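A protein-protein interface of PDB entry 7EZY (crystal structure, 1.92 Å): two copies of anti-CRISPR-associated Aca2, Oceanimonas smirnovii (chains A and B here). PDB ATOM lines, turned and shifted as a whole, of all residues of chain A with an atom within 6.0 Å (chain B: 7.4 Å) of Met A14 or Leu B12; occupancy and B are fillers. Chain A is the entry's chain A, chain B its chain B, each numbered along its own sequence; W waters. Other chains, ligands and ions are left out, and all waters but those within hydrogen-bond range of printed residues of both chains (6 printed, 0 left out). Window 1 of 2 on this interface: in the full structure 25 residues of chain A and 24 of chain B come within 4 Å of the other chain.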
ATOM      1  N   LEU A   9     -17.707 -17.270  16.830  1.00  0.00           N
ATOM      2  CA  LEU A   9     -16.934 -17.354  15.582  1.00  0.00           C
ATOM      3  C   LEU A   9     -15.551 -16.709  15.725  1.00  0.00           C
ATOM      4  O   LEU A   9     -14.551 -17.239  15.207  1.00  0.00           O
ATOM      5  CB  LEU A   9     -17.721 -16.711  14.440  1.00  0.00           C
ATOM      6  CG  LEU A   9     -19.026 -17.457  14.101  1.00  0.00           C
ATOM      7  CD1 LEU A   9     -19.755 -16.792  12.941  1.00  0.00           C
ATOM      8  CD2 LEU A   9     -18.755 -18.934  13.817  1.00  0.00           C
ATOM      9  N   ARG A  10     -15.479 -15.556  16.397  1.00  0.00           N
ATOM     10  CA  ARG A  10     -14.203 -14.887  16.592  1.00  0.00           C
ATOM     11  C   ARG A  10     -13.230 -15.800  17.327  1.00  0.00           C
ATOM     12  O   ARG A  10     -12.061 -15.881  16.956  1.00  0.00           O
ATOM     13  CB  ARG A  10     -14.398 -13.584  17.369  1.00  0.00           C
ATOM     14  CG  ARG A  10     -13.182 -12.653  17.421  1.00  0.00           C
ATOM     15  CD  ARG A  10     -12.231 -12.900  18.592  1.00  0.00           C
ATOM     16  NE  ARG A  10     -12.874 -12.882  19.908  1.00  0.00           N
ATOM     17  CZ  ARG A  10     -12.315 -13.355  21.009  1.00  0.00           C
ATOM     18  NH1 ARG A  10     -11.116 -13.911  20.984  1.00  0.00           N
ATOM     19  NH2 ARG A  10     -12.992 -13.297  22.163  1.00  0.00           N
ATOM     20  N   LYS A  11     -13.697 -16.498  18.377  1.00  0.00           N
ATOM     21  CA  LYS A  11     -12.825 -17.421  19.103  1.00  0.00           C
ATOM     22  C   LYS A  11     -12.456 -18.621  18.236  1.00  0.00           C
ATOM     23  O   LYS A  11     -11.307 -19.081  18.270  1.00  0.00           O
ATOM     24  CB  LYS A  11     -13.494 -17.904  20.413  1.00  0.00           C
ATOM     25  CG  LYS A  11     -13.690 -16.779  21.448  1.00  0.00           C
ATOM     26  CD  LYS A  11     -14.371 -17.319  22.728  1.00  0.00           C
ATOM     27  CE  LYS A  11     -13.336 -18.124  23.554  1.00  0.00           C
ATOM     28  NZ  LYS A  11     -12.386 -17.189  24.276  1.00  0.00           N
ATOM     29  N   LEU A  12     -13.426 -19.150  17.467  1.00  0.00           N
ATOM     30  CA  LEU A  12     -13.166 -20.315  16.614  1.00  0.00           C
ATOM     31  C   LEU A  12     -12.079 -20.032  15.588  1.00  0.00           C
ATOM     32  O   LEU A  12     -11.179 -20.857  15.360  1.00  0.00           O
ATOM     33  CB  LEU A  12     -14.445 -20.731  15.882  1.00  0.00           C
ATOM     34  CG  LEU A  12     -14.295 -22.059  15.124  1.00  0.00           C
ATOM     35  CD1 LEU A  12     -14.082 -23.221  16.059  1.00  0.00           C
ATOM     36  CD2 LEU A  12     -15.484 -22.319  14.244  1.00  0.00           C
ATOM     37  N   LEU A  13     -12.210 -18.915  14.885  1.00  0.00           N
ATOM     38  CA  LEU A  13     -11.087 -18.369  14.153  1.00  0.00           C
ATOM     39  C   LEU A  13     -10.120 -18.005  15.258  1.00  0.00           C
ATOM     40  O   LEU A  13     -10.546 -17.627  16.338  1.00  0.00           O
ATOM     41  CB  LEU A  13     -11.529 -17.134  13.365  1.00  0.00           C
ATOM     42  CG  LEU A  13     -12.725 -17.329  12.412  1.00  0.00           C
ATOM     43  CD1 LEU A  13     -13.382 -15.991  12.152  1.00  0.00           C
ATOM     44  CD2 LEU A  13     -12.353 -17.966  11.103  1.00  0.00           C
ATOM     45  N   MET A  14      -8.840 -18.167  15.112  1.00  0.00           N
ATOM     46  CA  MET A  14      -8.194 -18.024  16.430  1.00  0.00           C
ATOM     47  C   MET A  14      -7.710 -16.586  16.646  1.00  0.00           C
ATOM     48  O   MET A  14      -6.543 -16.270  16.910  1.00  0.00           O
ATOM     49  CB  MET A  14      -7.104 -19.052  16.652  1.00  0.00           C
ATOM     50  CG  MET A  14      -7.634 -20.471  16.695  1.00  0.00           C
ATOM     51  SD  MET A  14      -6.290 -21.641  16.763  1.00  0.00           S
ATOM     52  CE  MET A  14      -7.009 -22.975  17.734  1.00  0.00           C
ATOM     53  N   LEU A  15      -8.680 -15.691  16.571  1.00  0.00           N
ATOM     54  CA  LEU A  15      -8.416 -14.268  16.674  1.00  0.00           C
ATOM     55  C   LEU A  15      -8.390 -13.810  18.132  1.00  0.00           C
ATOM     56  O   LEU A  15      -9.289 -14.138  18.919  1.00  0.00           O
ATOM     57  CB  LEU A  15      -9.487 -13.497  15.915  1.00  0.00           C
ATOM     58  CG  LEU A  15      -9.338 -13.582  14.403  1.00  0.00           C
ATOM     59  CD1 LEU A  15     -10.622 -13.100  13.787  1.00  0.00           C
ATOM     60  CD2 LEU A  15      -8.165 -12.740  13.921  1.00  0.00           C
ATOM     61  N   GLU A  16      -7.400 -12.996  18.467  1.00  0.00           N
ATOM     62  CA  GLU A  16      -7.469 -12.259  19.717  1.00  0.00           C
ATOM     63  C   GLU A  16      -8.450 -11.086  19.571  1.00  0.00           C
ATOM     64  O   GLU A  16      -8.716 -10.601  18.473  1.00  0.00           O
ATOM     65  CB  GLU A  16      -6.068 -11.777  20.102  1.00  0.00           C
ATOM     66  CG  GLU A  16      -5.114 -12.927  20.402  1.00  0.00           C
ATOM     67  CD  GLU A  16      -5.494 -13.630  21.686  1.00  0.00           C
ATOM     68  OE1 GLU A  16      -5.554 -12.933  22.707  1.00  0.00           O
ATOM     69  OE2 GLU A  16      -5.793 -14.852  21.678  1.00  0.00           O
ATOM     70  N   GLU A  19      -6.800  -8.211  17.819  1.00  0.00           N
ATOM     71  CA  GLU A  19      -6.612  -8.441  16.391  1.00  0.00           C
ATOM     72  C   GLU A  19      -7.917  -8.272  15.636  1.00  0.00           C
ATOM     73  O   GLU A  19      -7.947  -7.627  14.589  1.00  0.00           O
ATOM     74  CB  GLU A  19      -6.033  -9.837  16.155  1.00  0.00           C
ATOM     75  CG  GLU A  19      -4.681 -10.051  16.848  1.00  0.00           C
ATOM     76  CD  GLU A  19      -4.323 -11.522  16.960  1.00  0.00           C
ATOM     77  OE1 GLU A  19      -5.227 -12.364  16.728  1.00  0.00           O
ATOM     78  OE2 GLU A  19      -3.161 -11.839  17.331  1.00  0.00           O
ATOM     79  N   ARG A  57     -12.445 -20.512   6.512  1.00  0.00           N
ATOM     80  CA  ARG A  57     -11.982 -21.635   7.329  1.00  0.00           C
ATOM     81  C   ARG A  57     -12.532 -22.941   6.762  1.00  0.00           C
ATOM     82  O   ARG A  57     -11.803 -23.937   6.616  1.00  0.00           O
ATOM     83  CB  ARG A  57     -12.419 -21.440   8.788  1.00  0.00           C
ATOM     84  CG  ARG A  57     -12.072 -22.599   9.702  1.00  0.00           C
ATOM     85  CD  ARG A  57     -12.704 -22.402  11.083  1.00  0.00           C
ATOM     86  NE  ARG A  57     -12.597 -23.590  11.920  1.00  0.00           N
ATOM     87  CZ  ARG A  57     -13.486 -24.573  11.942  1.00  0.00           C
ATOM     88  NH1 ARG A  57     -14.545 -24.562  11.151  1.00  0.00           N
ATOM     89  NH2 ARG A  57     -13.295 -25.606  12.757  1.00  0.00           N
ATOM     90  N   PHE A  79       2.355 -25.386  11.901  1.00  0.00           N
ATOM     91  CA  PHE A  79       1.672 -24.638  12.946  1.00  0.00           C
ATOM     92  C   PHE A  79       2.611 -23.506  13.318  1.00  0.00           C
ATOM     93  O   PHE A  79       3.651 -23.739  13.940  1.00  0.00           O
ATOM     94  CB  PHE A  79       1.337 -25.485  14.164  1.00  0.00           C
ATOM     95  CG  PHE A  79       0.453 -24.756  15.139  1.00  0.00           C
ATOM     96  CD1 PHE A  79      -0.928 -24.742  14.950  1.00  0.00           C
ATOM     97  CD2 PHE A  79       0.998 -24.018  16.187  1.00  0.00           C
ATOM     98  CE1 PHE A  79      -1.755 -24.020  15.817  1.00  0.00           C
ATOM     99  CE2 PHE A  79       0.173 -23.287  17.053  1.00  0.00           C
ATOM    100  CZ  PHE A  79      -1.192 -23.299  16.870  1.00  0.00           C
ATOM    101  N   ARG A  99      -3.865 -16.501  11.796  1.00  0.00           N
ATOM    102  CA  ARG A  99      -4.746 -17.175  12.746  1.00  0.00           C
ATOM    103  C   ARG A  99      -5.586 -18.247  12.046  1.00  0.00           C
ATOM    104  O   ARG A  99      -5.848 -19.309  12.621  1.00  0.00           O
ATOM    105  CB  ARG A  99      -5.651 -16.158  13.454  1.00  0.00           C
ATOM    106  CG  ARG A  99      -4.881 -15.132  14.337  1.00  0.00           C
ATOM    107  CD  ARG A  99      -3.959 -15.828  15.337  1.00  0.00           C
ATOM    108  NE  ARG A  99      -3.579 -14.972  16.465  1.00  0.00           N
ATOM    109  CZ  ARG A  99      -2.810 -15.358  17.473  1.00  0.00           C
ATOM    110  NH1 ARG A  99      -2.330 -16.583  17.538  1.00  0.00           N
ATOM    111  NH2 ARG A  99      -2.488 -14.475  18.423  1.00  0.00           N
ATOM    112  N   LEU A 100      -6.015 -17.984  10.809  1.00  0.00           N
ATOM    113  CA  LEU A 100      -6.770 -18.985  10.066  1.00  0.00           C
ATOM    114  C   LEU A 100      -5.957 -20.253   9.880  1.00  0.00           C
ATOM    115  O   LEU A 100      -6.498 -21.362   9.998  1.00  0.00           O
ATOM    116  CB  LEU A 100      -7.201 -18.435   8.705  1.00  0.00           C
ATOM    117  CG  LEU A 100      -8.602 -17.850   8.510  1.00  0.00           C
ATOM    118  CD1 LEU A 100      -8.669 -17.186   7.125  1.00  0.00           C
ATOM    119  CD2 LEU A 100      -9.674 -18.884   8.657  1.00  0.00           C
ATOM    120  N   GLN A 102      -3.697 -21.351  11.804  1.00  0.00           N
ATOM    121  CA  GLN A 102      -3.680 -22.018  13.110  1.00  0.00           C
ATOM    122  C   GLN A 102      -4.981 -22.767  13.371  1.00  0.00           C
ATOM    123  O   GLN A 102      -4.965 -23.900  13.853  1.00  0.00           O
ATOM    124  CB  GLN A 102      -3.426 -21.018  14.240  1.00  0.00           C
ATOM    125  CG  GLN A 102      -2.034 -20.397  14.250  1.00  0.00           C
ATOM    126  CD  GLN A 102      -1.824 -19.582  15.511  1.00  0.00           C
ATOM    127  OE1 GLN A 102      -2.719 -18.847  15.938  1.00  0.00           O
ATOM    128  NE2 GLN A 102      -0.657 -19.715  16.120  1.00  0.00           N
ATOM    129  N   ALA A 103      -6.119 -22.134  13.078  1.00  0.00           N
ATOM    130  CA  ALA A 103      -7.412 -22.764  13.353  1.00  0.00           C
ATOM    131  C   ALA A 103      -7.600 -24.040  12.521  1.00  0.00           C
ATOM    132  O   ALA A 103      -8.005 -25.094  13.041  1.00  0.00           O
ATOM    133  CB  ALA A 103      -8.538 -21.773  13.060  1.00  0.00           C
ATOM    134  N   ALA A 106      -4.975 -26.792  13.709  1.00  0.00           N
ATOM    135  CA  ALA A 106      -5.306 -27.337  15.014  1.00  0.00           C
ATOM    136  C   ALA A 106      -6.496 -28.277  14.924  1.00  0.00           C
ATOM    137  O   ALA A 106      -6.481 -29.362  15.536  1.00  0.00           O
ATOM    138  CB  ALA A 106      -5.595 -26.188  15.991  1.00  0.00           C
ATOM    139  N   THR A 107      -7.537 -27.874  14.171  1.00  0.00           N
ATOM    140  CA  THR A 107      -8.725 -28.717  14.036  1.00  0.00           C
ATOM    141  C   THR A 107      -8.381 -30.051  13.398  1.00  0.00           C
ATOM    142  O   THR A 107      -8.794 -31.107  13.889  1.00  0.00           O
ATOM    143  CB  THR A 107      -9.806 -28.022  13.203  1.00  0.00           C
ATOM    144  OG1 THR A 107     -10.021 -26.709  13.711  1.00  0.00           O
ATOM    145  CG2 THR A 107     -11.101 -28.768  13.366  1.00  0.00           C
ATOM    146  N   ALA A 110      -6.325 -32.271  15.798  1.00  0.00           N
ATOM    147  CA  ALA A 110      -7.108 -32.904  16.866  1.00  0.00           C
ATOM    148  C   ALA A 110      -7.929 -34.069  16.328  1.00  0.00           C
ATOM    149  O   ALA A 110      -8.047 -35.117  16.983  1.00  0.00           O
ATOM    150  CB  ALA A 110      -8.043 -31.897  17.518  1.00  0.00           C
ATOM    151  N   LEU B   6       1.088 -29.056  21.723  1.00  0.00           N
ATOM    152  CA  LEU B   6       0.449 -28.611  22.955  1.00  0.00           C
ATOM    153  C   LEU B   6      -0.297 -27.298  22.744  1.00  0.00           C
ATOM    154  O   LEU B   6      -1.462 -27.159  23.145  1.00  0.00           O
ATOM    155  CB  LEU B   6       1.501 -28.450  24.048  1.00  0.00           C
ATOM    156  CG  LEU B   6       0.982 -27.848  25.346  1.00  0.00           C
ATOM    157  CD1 LEU B   6       0.018 -28.825  26.010  1.00  0.00           C
ATOM    158  CD2 LEU B   6       2.121 -27.508  26.284  1.00  0.00           C
ATOM    159  N   GLN B   7       0.363 -26.318  22.121  1.00  0.00           N
ATOM    160  CA  GLN B   7      -0.285 -25.025  21.907  1.00  0.00           C
ATOM    161  C   GLN B   7      -1.514 -25.145  21.003  1.00  0.00           C
ATOM    162  O   GLN B   7      -2.554 -24.520  21.268  1.00  0.00           O
ATOM    163  CB  GLN B   7       0.695 -24.026  21.301  1.00  0.00           C
ATOM    164  CG  GLN B   7       0.118 -22.628  21.268  1.00  0.00           C
ATOM    165  CD  GLN B   7       1.124 -21.605  20.860  1.00  0.00           C
ATOM    166  OE1 GLN B   7       1.424 -21.463  19.663  1.00  0.00           O
ATOM    167  NE2 GLN B   7       1.630 -20.842  21.836  1.00  0.00           N
ATOM    168  N   ALA B   8      -1.402 -25.897  19.907  1.00  0.00           N
ATOM    169  CA  ALA B   8      -2.521 -26.041  18.981  1.00  0.00           C
ATOM    170  C   ALA B   8      -3.747 -26.618  19.688  1.00  0.00           C
ATOM    171  O   ALA B   8      -4.871 -26.114  19.528  1.00  0.00           O
ATOM    172  CB  ALA B   8      -2.103 -26.928  17.805  1.00  0.00           C
ATOM    173  N   LEU B   9      -3.548 -27.668  20.484  1.00  0.00           N
ATOM    174  CA  LEU B   9      -4.683 -28.271  21.192  1.00  0.00           C
ATOM    175  C   LEU B   9      -5.208 -27.341  22.276  1.00  0.00           C
ATOM    176  O   LEU B   9      -6.429 -27.195  22.442  1.00  0.00           O
ATOM    177  CB  LEU B   9      -4.273 -29.622  21.792  1.00  0.00           C
ATOM    178  CG  LEU B   9      -3.919 -30.682  20.739  1.00  0.00           C
ATOM    179  CD1 LEU B   9      -3.430 -31.956  21.409  1.00  0.00           C
ATOM    180  CD2 LEU B   9      -5.131 -30.961  19.848  1.00  0.00           C
ATOM    181  N   ARG B  10      -4.301 -26.704  23.021  1.00  0.00           N
ATOM    182  CA  ARG B  10      -4.725 -25.782  24.062  1.00  0.00           C
ATOM    183  C   ARG B  10      -5.600 -24.684  23.483  1.00  0.00           C
ATOM    184  O   ARG B  10      -6.634 -24.344  24.067  1.00  0.00           O
ATOM    185  CB  ARG B  10      -3.497 -25.180  24.760  1.00  0.00           C
ATOM    186  CG  ARG B  10      -3.823 -24.412  26.028  1.00  0.00           C
ATOM    187  CD  ARG B  10      -3.999 -22.902  25.802  1.00  0.00           C
ATOM    188  NE  ARG B  10      -2.877 -22.257  25.109  1.00  0.00           N
ATOM    189  CZ  ARG B  10      -2.965 -21.064  24.538  1.00  0.00           C
ATOM    190  NH1 ARG B  10      -4.104 -20.394  24.529  1.00  0.00           N
ATOM    191  NH2 ARG B  10      -1.888 -20.535  23.958  1.00  0.00           N
ATOM    192  N   LYS B  11      -5.205 -24.131  22.331  1.00  0.00           N
ATOM    193  CA  LYS B  11      -5.988 -23.081  21.688  1.00  0.00           C
ATOM    194  C   LYS B  11      -7.296 -23.625  21.126  1.00  0.00           C
ATOM    195  O   LYS B  11      -8.330 -22.956  21.203  1.00  0.00           O
ATOM    196  CB  LYS B  11      -5.181 -22.409  20.574  1.00  0.00           C
ATOM    197  CG  LYS B  11      -3.973 -21.585  21.055  1.00  0.00           C
ATOM    198  CD  LYS B  11      -3.189 -21.018  19.870  1.00  0.00           C
ATOM    199  CE  LYS B  11      -3.909 -19.859  19.156  1.00  0.00           C
ATOM    200  NZ  LYS B  11      -3.924 -18.598  19.979  1.00  0.00           N
ATOM    201  N   LEU B  12      -7.262 -24.814  20.526  1.00  0.00           N
ATOM    202  CA  LEU B  12      -8.475 -25.410  19.965  1.00  0.00           C
ATOM    203  C   LEU B  12      -9.505 -25.646  21.059  1.00  0.00           C
ATOM    204  O   LEU B  12     -10.703 -25.364  20.881  1.00  0.00           O
ATOM    205  CB  LEU B  12      -8.139 -26.721  19.254  1.00  0.00           C
ATOM    206  CG  LEU B  12      -9.365 -27.306  18.530  1.00  0.00           C
ATOM    207  CD1 LEU B  12      -9.764 -26.506  17.268  1.00  0.00           C
ATOM    208  CD2 LEU B  12      -9.164 -28.762  18.239  1.00  0.00           C
ATOM    209  N   LEU B  13      -9.056 -26.208  22.186  1.00  0.00           N
ATOM    210  CA  LEU B  13      -9.831 -26.114  23.404  1.00  0.00           C
ATOM    211  C   LEU B  13      -9.852 -24.630  23.694  1.00  0.00           C
ATOM    212  O   LEU B  13      -8.907 -23.924  23.384  1.00  0.00           O
ATOM    213  CB  LEU B  13      -9.155 -26.887  24.544  1.00  0.00           C
ATOM    214  CG  LEU B  13      -8.842 -28.343  24.173  1.00  0.00           C
ATOM    215  CD1 LEU B  13      -7.879 -28.976  25.144  1.00  0.00           C
ATOM    216  CD2 LEU B  13     -10.087 -29.204  24.027  1.00  0.00           C
ATOM    217  N   MET B  14     -10.914 -24.080  24.195  1.00  0.00           N
ATOM    218  CA  MET B  14     -10.690 -22.627  24.094  1.00  0.00           C
ATOM    219  C   MET B  14     -10.066 -22.099  25.386  1.00  0.00           C
ATOM    220  O   MET B  14     -10.587 -21.197  26.042  1.00  0.00           O
ATOM    221  CB  MET B  14     -11.988 -21.900  23.757  1.00  0.00           C
ATOM    222  CG  MET B  14     -12.167 -21.620  22.233  1.00  0.00           C
ATOM    223  SD  MET B  14     -13.899 -21.606  21.860  1.00  0.00           S
ATOM    224  CE  MET B  14     -13.873 -21.551  20.050  1.00  0.00           C
ATOM    225  N   LEU B  15      -8.923 -22.677  25.773  1.00  0.00           N
ATOM    226  CA  LEU B  15      -8.292 -22.368  27.053  1.00  0.00           C
ATOM    227  C   LEU B  15      -7.365 -21.170  26.935  1.00  0.00           C
ATOM    228  O   LEU B  15      -6.636 -21.044  25.954  1.00  0.00           O
ATOM    229  CB  LEU B  15      -7.493 -23.580  27.542  1.00  0.00           C
ATOM    230  CG  LEU B  15      -8.360 -24.731  28.067  1.00  0.00           C
ATOM    231  CD1 LEU B  15      -7.519 -25.985  28.180  1.00  0.00           C
ATOM    232  CD2 LEU B  15      -9.001 -24.380  29.405  1.00  0.00           C
ATOM    233  N   THR B  54      -9.009 -33.351  24.469  1.00  0.00           N
ATOM    234  CA  THR B  54      -9.288 -33.381  23.030  1.00  0.00           C
ATOM    235  C   THR B  54     -10.248 -34.524  22.673  1.00  0.00           C
ATOM    236  O   THR B  54     -11.156 -34.359  21.838  1.00  0.00           O
ATOM    237  CB  THR B  54      -7.968 -33.503  22.251  1.00  0.00           C
ATOM    238  OG1 THR B  54      -7.078 -32.427  22.615  1.00  0.00           O
ATOM    239  CG2 THR B  54      -8.217 -33.480  20.758  1.00  0.00           C
ATOM    240  N   ARG B  57     -13.633 -33.425  23.632  1.00  0.00           N
ATOM    241  CA  ARG B  57     -14.177 -32.541  22.606  1.00  0.00           C
ATOM    242  C   ARG B  57     -14.799 -33.342  21.478  1.00  0.00           C
ATOM    243  O   ARG B  57     -15.944 -33.090  21.065  1.00  0.00           O
ATOM    244  CB  ARG B  57     -13.078 -31.635  22.059  1.00  0.00           C
ATOM    245  CG  ARG B  57     -13.540 -30.724  20.941  1.00  0.00           C
ATOM    246  CD  ARG B  57     -12.359 -29.961  20.315  1.00  0.00           C
ATOM    247  NE  ARG B  57     -12.732 -29.263  19.095  1.00  0.00           N
ATOM    248  CZ  ARG B  57     -12.731 -29.824  17.896  1.00  0.00           C
ATOM    249  NH1 ARG B  57     -12.422 -31.102  17.735  1.00  0.00           N
ATOM    250  NH2 ARG B  57     -13.032 -29.084  16.834  1.00  0.00           N
ATOM    251  N   ARG B  99     -14.846 -24.029  28.872  1.00  0.00           N
ATOM    252  CA  ARG B  99     -14.164 -23.748  27.610  1.00  0.00           C
ATOM    253  C   ARG B  99     -14.466 -24.826  26.577  1.00  0.00           C
ATOM    254  O   ARG B  99     -14.668 -24.525  25.392  1.00  0.00           O
ATOM    255  CB  ARG B  99     -12.656 -23.644  27.870  1.00  0.00           C
ATOM    256  CG  ARG B  99     -12.257 -22.446  28.709  1.00  0.00           C
ATOM    257  CD  ARG B  99     -12.822 -21.127  28.164  1.00  0.00           C
ATOM    258  NE  ARG B  99     -12.079 -19.969  28.662  1.00  0.00           N
ATOM    259  CZ  ARG B  99     -12.384 -18.705  28.405  1.00  0.00           C
ATOM    260  NH1 ARG B  99     -13.393 -18.388  27.605  1.00  0.00           N
ATOM    261  NH2 ARG B  99     -11.673 -17.731  28.984  1.00  0.00           N
ATOM    262  N   LEU B 100     -14.537 -26.088  27.021  1.00  0.00           N
ATOM    263  CA  LEU B 100     -14.919 -27.181  26.125  1.00  0.00           C
ATOM    264  C   LEU B 100     -16.317 -26.980  25.533  1.00  0.00           C
ATOM    265  O   LEU B 100     -16.535 -27.247  24.339  1.00  0.00           O
ATOM    266  CB  LEU B 100     -14.840 -28.512  26.878  1.00  0.00           C
ATOM    267  CG  LEU B 100     -13.716 -29.479  26.554  1.00  0.00           C
ATOM    268  CD1 LEU B 100     -14.077 -30.846  27.035  1.00  0.00           C
ATOM    269  CD2 LEU B 100     -13.563 -29.506  25.043  1.00  0.00           C
ATOM    270  N   GLN B 102     -17.737 -24.181  24.997  1.00  0.00           N
ATOM    271  CA  GLN B 102     -17.591 -23.106  24.011  1.00  0.00           C
ATOM    272  C   GLN B 102     -17.032 -23.633  22.699  1.00  0.00           C
ATOM    273  O   GLN B 102     -17.491 -23.249  21.622  1.00  0.00           O
ATOM    274  CB  GLN B 102     -16.683 -22.003  24.534  1.00  0.00           C
ATOM    275  CG  GLN B 102     -17.247 -21.214  25.688  1.00  0.00           C
ATOM    276  CD  GLN B 102     -16.424 -19.992  25.992  1.00  0.00           C
ATOM    277  OE1 GLN B 102     -15.189 -20.051  25.988  1.00  0.00           O
ATOM    278  NE2 GLN B 102     -17.100 -18.852  26.234  1.00  0.00           N
ATOM    279  N   ALA B 103     -15.988 -24.465  22.775  1.00  0.00           N
ATOM    280  CA  ALA B 103     -15.343 -24.968  21.559  1.00  0.00           C
ATOM    281  C   ALA B 103     -16.293 -25.860  20.747  1.00  0.00           C
ATOM    282  O   ALA B 103     -16.371 -25.752  19.510  1.00  0.00           O
ATOM    283  CB  ALA B 103     -14.073 -25.729  21.928  1.00  0.00           C
ATOM    284  N   VAL B 104     -17.017 -26.750  21.430  1.00  0.00           N
ATOM    285  CA  VAL B 104     -17.967 -27.626  20.747  1.00  0.00           C
ATOM    286  C   VAL B 104     -19.051 -26.792  20.088  1.00  0.00           C
ATOM    287  O   VAL B 104     -19.390 -26.985  18.901  1.00  0.00           O
ATOM    288  CB  VAL B 104     -18.573 -28.641  21.731  1.00  0.00           C
ATOM    289  CG1 VAL B 104     -19.817 -29.353  21.119  1.00  0.00           C
ATOM    290  CG2 VAL B 104     -17.538 -29.627  22.220  1.00  0.00           C
ATOM    291  N   THR B 107     -17.763 -24.759  17.016  1.00  0.00           N
ATOM    292  CA  THR B 107     -17.536 -25.537  15.785  1.00  0.00           C
ATOM    293  C   THR B 107     -18.861 -25.914  15.122  1.00  0.00           C
ATOM    294  O   THR B 107     -19.036 -25.754  13.899  1.00  0.00           O
ATOM    295  CB  THR B 107     -16.717 -26.806  16.024  1.00  0.00           C
ATOM    296  OG1 THR B 107     -15.719 -26.565  17.011  1.00  0.00           O
ATOM    297  CG2 THR B 107     -15.986 -27.137  14.725  1.00  0.00           C
HETATM  298  O   HOH W   1       0.593 -19.031  18.590  1.00  0.00           O
HETATM  299  O   HOH W   2     -10.294 -22.063  19.033  1.00  0.00           O
HETATM  300  O   HOH W   3     -10.547 -18.588  25.622  1.00  0.00           O
HETATM  301  O   HOH W   4     -13.789 -15.561  26.160  1.00  0.00           O
HETATM  302  O   HOH W   5      -5.484 -16.683  19.493  1.00  0.00           O
HETATM  303  O   HOH W   6      -0.928 -17.914  20.289  1.00  0.00           O
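The backbone carbonyl oxygen of Met B14 sits close to the guanidinium group of Arg B99 (3.3 Å).
NH1 of Arg A99 is in hydrogen-bond range of OE1 of Gln A102.
The guanidinium group (NE) of Arg A99 lies close to the backbone carbonyl oxygen (O) of Met A14.
The side-chain amide oxygen (OE1) of Gln B102 lies within hydrogen-bond range of the guanidinium group (NH1) of Arg B99 (2.9 Å).
The backbone carbonyl oxygen (O) of Ala B103 lies within hydrogen-bond range of the side-chain hydroxyl (OG1) of Thr B107 (2.7 Å).
N of Ala B103 lies within hydrogen-bond range of SD of Met B14.
Lys A11 touches Met B14 (CB to CE, 3.7 Å).
NH1 of Arg B99 touches NZ of Lys A11 (3.7 Å).
CB of Lys B11 touches CE of Met A14, 3.4 Å away.
Ala B8 touches Phe A79.
Ala A106 touches Leu B12 (O to CD2, 3.9 Å).
Thr A107 touches Leu B12 (OG1 to CD1, 3.6 Å).
Arg B57 touches Thr A107 (NH2 to CG2, 3.98 Å).
Ala A110 touches Leu B9.
CD2 of Leu B12 touches CB of Ala A110, 3.4 Å away.
Ala A110 touches Thr B54.
Of the printed residues of chain B, Met A14 touches Lys B11 and Leu B12.
Leu B12 touches just these residues of chain A: Met A14 (3.4 Å), Ala A106 (3.9 Å), Thr A107 (3.6 Å) and Ala A110 (3.4 Å).
Of the printed residues of chain B, Leu A12 touches Met B14 (3.6 Å) and Thr B107 (3.8 Å).
Of the printed residues of chain A, Thr B107 touches Leu A12 and Arg A57.
Of the printed residues of chain A, Gln B102 touches Lys A11.
Printed residues of chain B within 4 Å of Gln A102: Lys B11 (3.6 Å).
The nearest residue of chain A that does not touch Leu B12 is Ala A103 (4.8 Å).
Hydrophobic or aromatic side chains of chain A within 4 Å of the printed part of chain B: Leu A12, Met A14, Phe A79, Ala A106 and Ala A110.
Along chain A the printed residues that touch a printed residue of chain B span positions 11 to 110.
Of the 18 printed residues of chain B, 11 touch a printed residue of chain A.
Hydrophobic or aromatic side chains of chain B within 4 Å of the printed part of chain A: Ala B8, Leu B9, Leu B12 and Met B14.
Among the printed residues, no Asp or Glu carboxylate lies within 4 Å of a Lys or Arg side-chain nitrogen of the other chain.
Lys A11 touches Met B14, and with the chains exchanged Met A14 touches Lys B11.
Lys A11 touches Arg B99, and with the chains exchanged Arg A99 touches Lys B11.
Lys A11 touches Gln B102, and with the chains exchanged Gln A102 touches Lys B11.
Leu A12 touches Met B14, and with the chains exchanged Met A14 touches Leu B12.
13 positions are printed for both chains.
Of the 19 pairs that touch across the chains among the printed residues, 12 have their exchanged pair printed and touching as well.
Water W5 lies within hydrogen-bond range of NZ of Lys B11 (2.5 Å), O of Met A14 (2.8 Å) and OE2 of Glu A16 (2.9 Å).
Water W3 lies within hydrogen-bond range of the backbone carbonyl oxygen of Met B14 (2.6 Å), the side-chain amino group of Lys A11 (2.7 Å) and the guanidinium group of Arg B99 (3.5 Å).
Water W1 lies within hydrogen-bond range of OE1 of Gln B7 (2.8 Å) and NE2 of Gln A102 (2.9 Å).
Water W4 bridges the side-chain amino group (NZ) of Lys A11 (2.9 Å) and the guanidinium group (NH1) of Arg B99 (3.2 Å).
Water W2 bridges O of Lys B11 (3.1 Å) and O of Lys A11 (3.2 Å).
Water W6 bridges NZ of Lys B11 (3.1 Å) and NH1 of Arg A99 (3.4 Å).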
